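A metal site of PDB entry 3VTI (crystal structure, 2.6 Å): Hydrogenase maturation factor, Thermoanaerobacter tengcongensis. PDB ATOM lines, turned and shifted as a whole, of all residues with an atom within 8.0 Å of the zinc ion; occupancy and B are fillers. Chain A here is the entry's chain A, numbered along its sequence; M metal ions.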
ATOM      1  N   MET A 111      15.723 -26.008  15.500  1.00  0.00           N
ATOM      2  CA  MET A 111      16.553 -26.323  14.328  1.00  0.00           C
ATOM      3  C   MET A 111      17.104 -27.750  14.326  1.00  0.00           C
ATOM      4  O   MET A 111      17.596 -28.253  15.337  1.00  0.00           O
ATOM      5  CB  MET A 111      17.708 -25.332  14.181  1.00  0.00           C
ATOM      6  CG  MET A 111      17.313 -23.943  13.669  1.00  0.00           C
ATOM      7  SD  MET A 111      18.650 -22.719  13.830  1.00  0.00           S
ATOM      8  CE  MET A 111      18.691 -22.457  15.614  1.00  0.00           C
ATOM      9  N   GLY A 112      17.043 -28.371  13.143  1.00  0.00           N
ATOM     10  CA  GLY A 112      17.631 -29.672  12.928  1.00  0.00           C
ATOM     11  C   GLY A 112      19.135 -29.593  13.079  1.00  0.00           C
ATOM     12  O   GLY A 112      19.714 -28.510  12.928  1.00  0.00           O
ATOM     13  N   VAL A 113      19.763 -30.727  13.383  1.00  0.00           N
ATOM     14  CA  VAL A 113      21.218 -30.813  13.527  1.00  0.00           C
ATOM     15  C   VAL A 113      21.940 -30.221  12.299  1.00  0.00           C
ATOM     16  O   VAL A 113      21.647 -30.595  11.166  1.00  0.00           O
ATOM     17  CB  VAL A 113      21.680 -32.291  13.732  1.00  0.00           C
ATOM     18  CG1 VAL A 113      23.066 -32.339  14.343  1.00  0.00           C
ATOM     19  CG2 VAL A 113      20.699 -33.057  14.609  1.00  0.00           C
ATOM     20  N   CYS A 114      22.876 -29.306  12.540  1.00  0.00           N
ATOM     21  CA  CYS A 114      23.663 -28.690  11.457  1.00  0.00           C
ATOM     22  C   CYS A 114      24.766 -29.636  11.022  1.00  0.00           C
ATOM     23  O   CYS A 114      25.094 -30.584  11.733  1.00  0.00           O
ATOM     24  CB  CYS A 114      24.278 -27.367  11.917  1.00  0.00           C
ATOM     25  SG  CYS A 114      25.667 -27.514  13.079  1.00  0.00           S
ATOM     26  N   GLU A 115      25.372 -29.342   9.882  1.00  0.00           N
ATOM     27  CA  GLU A 115      26.425 -30.182   9.301  1.00  0.00           C
ATOM     28  C   GLU A 115      27.648 -30.392  10.235  1.00  0.00           C
ATOM     29  O   GLU A 115      28.164 -31.494  10.358  1.00  0.00           O
ATOM     30  CB  GLU A 115      26.845 -29.658   7.926  1.00  0.00           C
ATOM     31  CG  GLU A 115      27.670 -30.635   7.092  1.00  0.00           C
ATOM     32  CD  GLU A 115      26.828 -31.653   6.280  1.00  0.00           C
ATOM     33  OE1 GLU A 115      25.619 -31.873   6.597  1.00  0.00           O
ATOM     34  OE2 GLU A 115      27.385 -32.219   5.310  1.00  0.00           O
ATOM     35  N   ASP A 116      28.090 -29.322  10.898  1.00  0.00           N
ATOM     36  CA  ASP A 116      29.226 -29.402  11.830  1.00  0.00           C
ATOM     37  C   ASP A 116      28.977 -30.287  13.058  1.00  0.00           C
ATOM     38  O   ASP A 116      29.839 -31.083  13.426  1.00  0.00           O
ATOM     39  CB  ASP A 116      29.646 -28.008  12.276  1.00  0.00           C
ATOM     40  CG  ASP A 116      29.886 -27.071  11.118  1.00  0.00           C
ATOM     41  OD1 ASP A 116      30.730 -27.387  10.246  1.00  0.00           O
ATOM     42  OD2 ASP A 116      29.231 -26.005  11.076  1.00  0.00           O
ATOM     43  N   CYS A 117      27.811 -30.149  13.674  1.00  0.00           N
ATOM     44  CA  CYS A 117      27.415 -31.008  14.795  1.00  0.00           C
ATOM     45  C   CYS A 117      27.289 -32.464  14.325  1.00  0.00           C
ATOM     46  O   CYS A 117      27.652 -33.386  15.053  1.00  0.00           O
ATOM     47  CB  CYS A 117      26.105 -30.532  15.434  1.00  0.00           C
ATOM     48  SG  CYS A 117      26.268 -29.098  16.523  1.00  0.00           S
ATOM     49  N   LEU A 118      26.788 -32.645  13.110  1.00  0.00           N
ATOM     50  CA  LEU A 118      26.676 -33.982  12.519  1.00  0.00           C
ATOM     51  C   LEU A 118      28.046 -34.644  12.375  1.00  0.00           C
ATOM     52  O   LEU A 118      28.213 -35.797  12.747  1.00  0.00           O
ATOM     53  CB  LEU A 118      25.976 -33.930  11.151  1.00  0.00           C
ATOM     54  CG  LEU A 118      25.365 -35.273  10.771  1.00  0.00           C
ATOM     55  CD1 LEU A 118      24.344 -35.633  11.854  1.00  0.00           C
ATOM     56  CD2 LEU A 118      24.718 -35.278   9.378  1.00  0.00           C
ATOM     57  N   GLU A 120      30.702 -33.840  14.073  1.00  0.00           N
ATOM     58  CA  GLU A 120      31.249 -34.076  15.413  1.00  0.00           C
ATOM     59  C   GLU A 120      30.582 -35.260  16.121  1.00  0.00           C
ATOM     60  O   GLU A 120      31.252 -36.024  16.816  1.00  0.00           O
ATOM     61  CB  GLU A 120      31.151 -32.826  16.270  1.00  0.00           C
ATOM     62  CG  GLU A 120      32.125 -31.726  15.857  1.00  0.00           C
ATOM     63  CD  GLU A 120      31.944 -30.467  16.672  1.00  0.00           C
ATOM     64  OE1 GLU A 120      32.813 -29.575  16.607  1.00  0.00           O
ATOM     65  OE2 GLU A 120      30.932 -30.375  17.386  1.00  0.00           O
ATOM     66  N   ILE A 134      23.763 -33.158  21.315  1.00  0.00           N
ATOM     67  CA  ILE A 134      24.738 -32.270  20.700  1.00  0.00           C
ATOM     68  C   ILE A 134      24.015 -31.138  19.972  1.00  0.00           C
ATOM     69  O   ILE A 134      23.045 -31.357  19.256  1.00  0.00           O
ATOM     70  CB  ILE A 134      25.697 -33.060  19.766  1.00  0.00           C
ATOM     71  CG1 ILE A 134      26.909 -32.197  19.373  1.00  0.00           C
ATOM     72  CG2 ILE A 134      24.972 -33.619  18.537  1.00  0.00           C
ATOM     73  CD1 ILE A 134      27.950 -32.956  18.543  1.00  0.00           C
ATOM     74  N   ASN A 135      24.506 -29.923  20.181  1.00  0.00           N
ATOM     75  CA  ASN A 135      23.987 -28.732  19.517  1.00  0.00           C
ATOM     76  C   ASN A 135      25.045 -27.639  19.529  1.00  0.00           C
ATOM     77  O   ASN A 135      26.065 -27.768  20.219  1.00  0.00           O
ATOM     78  CB  ASN A 135      22.714 -28.230  20.204  1.00  0.00           C
ATOM     79  CG  ASN A 135      22.964 -27.841  21.651  1.00  0.00           C
ATOM     80  OD1 ASN A 135      22.738 -28.648  22.557  1.00  0.00           O
ATOM     81  ND2 ASN A 135      23.448 -26.615  21.870  1.00  0.00           N
ATOM     82  N   CYS A 136      24.824 -26.582  18.750  1.00  0.00           N
ATOM     83  CA  CYS A 136      25.726 -25.422  18.735  1.00  0.00           C
ATOM     84  C   CYS A 136      24.915 -24.158  18.496  1.00  0.00           C
ATOM     85  O   CYS A 136      23.694 -24.187  18.533  1.00  0.00           O
ATOM     86  CB  CYS A 136      26.822 -25.594  17.673  1.00  0.00           C
ATOM     87  SG  CYS A 136      26.249 -25.507  15.963  1.00  0.00           S
ATOM     88  N   THR A 137      25.602 -23.046  18.257  1.00  0.00           N
ATOM     89  CA  THR A 137      24.943 -21.769  18.006  1.00  0.00           C
ATOM     90  C   THR A 137      24.021 -21.813  16.775  1.00  0.00           C
ATOM     91  O   THR A 137      23.091 -21.009  16.664  1.00  0.00           O
ATOM     92  CB  THR A 137      25.960 -20.592  17.891  1.00  0.00           C
ATOM     93  OG1 THR A 137      25.259 -19.349  17.924  1.00  0.00           O
ATOM     94  CG2 THR A 137      26.754 -20.661  16.583  1.00  0.00           C
ATOM     95  N   ASN A 138      24.269 -22.758  15.867  1.00  0.00           N
ATOM     96  CA  ASN A 138      23.550 -22.855  14.590  1.00  0.00           C
ATOM     97  C   ASN A 138      22.474 -23.966  14.499  1.00  0.00           C
ATOM     98  O   ASN A 138      21.811 -24.098  13.468  1.00  0.00           O
ATOM     99  CB  ASN A 138      24.561 -22.998  13.435  1.00  0.00           C
ATOM    100  CG  ASN A 138      25.479 -21.790  13.308  1.00  0.00           C
ATOM    101  OD1 ASN A 138      25.067 -20.658  13.558  1.00  0.00           O
ATOM    102  ND2 ASN A 138      26.733 -22.028  12.905  1.00  0.00           N
ATOM    103  N   CYS A 139      22.301 -24.759  15.552  1.00  0.00           N
ATOM    104  CA  CYS A 139      21.290 -25.806  15.557  1.00  0.00           C
ATOM    105  C   CYS A 139      20.764 -26.107  16.941  1.00  0.00           C
ATOM    106  O   CYS A 139      21.183 -25.496  17.935  1.00  0.00           O
ATOM    107  CB  CYS A 139      21.824 -27.083  14.894  1.00  0.00           C
ATOM    108  SG  CYS A 139      23.030 -28.025  15.846  1.00  0.00           S
ATOM    109  N   GLY A 140      19.826 -27.072  17.001  1.00  0.00           N
ATOM    110  CA  GLY A 140      19.326 -27.597  18.262  1.00  0.00           C
ATOM    111  C   GLY A 140      17.990 -26.979  18.633  1.00  0.00           C
ATOM    112  O   GLY A 140      17.399 -26.253  17.832  1.00  0.00           O
ATOM    113  N   ARG A 142      15.265 -24.547  20.230  1.00  0.00           N
ATOM    114  CA  ARG A 142      15.112 -23.151  20.582  1.00  0.00           C
ATOM    115  C   ARG A 142      13.746 -23.001  21.214  1.00  0.00           C
ATOM    116  O   ARG A 142      13.589 -23.293  22.408  1.00  0.00           O
ATOM    117  CB  ARG A 142      15.291 -22.259  19.359  1.00  0.00           C
ATOM    118  CG  ARG A 142      16.682 -22.280  18.735  1.00  0.00           C
ATOM    119  CD  ARG A 142      17.748 -21.709  19.676  1.00  0.00           C
ATOM    120  NE  ARG A 142      19.068 -21.723  19.039  1.00  0.00           N
ATOM    121  CZ  ARG A 142      19.901 -22.769  19.016  1.00  0.00           C
ATOM    122  NH1 ARG A 142      19.562 -23.917  19.609  1.00  0.00           N
ATOM    123  NH2 ARG A 142      21.061 -22.675  18.392  1.00  0.00           N
ATOM    124  N   ARG A 177      32.122 -22.174  17.859  1.00  0.00           N
ATOM    125  CA  ARG A 177      30.806 -22.416  17.251  1.00  0.00           C
ATOM    126  C   ARG A 177      29.725 -22.658  18.310  1.00  0.00           C
ATOM    127  O   ARG A 177      28.538 -22.751  17.983  1.00  0.00           O
ATOM    128  CB  ARG A 177      30.882 -23.584  16.265  1.00  0.00           C
ATOM    129  CG  ARG A 177      29.852 -23.505  15.154  1.00  0.00           C
ATOM    130  CD  ARG A 177      29.820 -24.752  14.307  1.00  0.00           C
ATOM    131  NE  ARG A 177      29.236 -25.903  14.989  1.00  0.00           N
ATOM    132  CZ  ARG A 177      29.933 -26.883  15.570  1.00  0.00           C
ATOM    133  NH1 ARG A 177      31.268 -26.846  15.553  1.00  0.00           N
ATOM    134  NH2 ARG A 177      29.305 -27.899  16.156  1.00  0.00           N
ATOM    135  N   ARG A 178      30.130 -22.748  19.571  1.00  0.00           N
ATOM    136  CA  ARG A 178      29.199 -22.855  20.688  1.00  0.00           C
ATOM    137  C   ARG A 178      29.164 -21.612  21.581  1.00  0.00           C
ATOM    138  O   ARG A 178      28.623 -21.661  22.697  1.00  0.00           O
ATOM    139  CB  ARG A 178      29.436 -24.146  21.484  1.00  0.00           C
ATOM    140  CG  ARG A 178      28.740 -25.350  20.851  1.00  0.00           C
ATOM    141  CD  ARG A 178      29.147 -26.680  21.433  1.00  0.00           C
ATOM    142  NE  ARG A 178      30.270 -27.226  20.697  1.00  0.00           N
ATOM    143  CZ  ARG A 178      30.174 -28.124  19.717  1.00  0.00           C
ATOM    144  NH1 ARG A 178      28.992 -28.590  19.327  1.00  0.00           N
ATOM    145  NH2 ARG A 178      31.272 -28.536  19.125  1.00  0.00           N
ATOM    146  N   GLN A 279      16.868 -27.201   7.546  1.00  0.00           N
ATOM    147  CA  GLN A 279      17.071 -27.340   8.994  1.00  0.00           C
ATOM    148  C   GLN A 279      15.739 -27.224   9.713  1.00  0.00           C
ATOM    149  O   GLN A 279      15.608 -27.618  10.865  1.00  0.00           O
ATOM    150  CB  GLN A 279      18.043 -26.307   9.514  1.00  0.00           C
ATOM    151  CG  GLN A 279      19.253 -26.919  10.206  1.00  0.00           C
ATOM    152  CD  GLN A 279      20.164 -25.859  10.811  1.00  0.00           C
ATOM    153  OE1 GLN A 279      20.613 -24.934  10.128  1.00  0.00           O
ATOM    154  NE2 GLN A 279      20.445 -25.996  12.102  1.00  0.00           N
HETATM  155 ZN    ZN M   1      25.160 -27.443  15.327  1.00  0.00          ZN
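NH1 of Arg 142 lies within hydrogen-bond range of O of Cys 139, 2.8 Å away. The backbone NH (N) of Asp 116 lies close to the side-chain sulfur (SG) of Cys 114, 3.7 Å away. The side-chain sulfur of Cys 136 sits close to the guanidinium group of Arg 177 (3.2 Å). SG of Cys 136 lies close to N of Asn 138, 3.4 Å away. The backbone carbonyl oxygen (O) of Cys 136 sits at hydrogen-bond distance from the guanidinium group (NH2) of Arg 142. SG of Cys 117 sits close to NH2 of Arg 177 (3.3 Å).
The zinc ion is bound by SG of Cys 139 (2.3 Å), SG of Cys 114 (2.3 Å), SG of Cys 136 (2.3 Å) and SG of Cys 117 (2.3 Å). The zinc ion has four donor atoms within binding distance.
Four residues have an atom within 4 Å of the zinc ion: Cys 114, Cys 117, Cys 136 and Cys 139. The nearest printed residue that does not touch the zinc ion is Asn 135 (4.2 Å).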
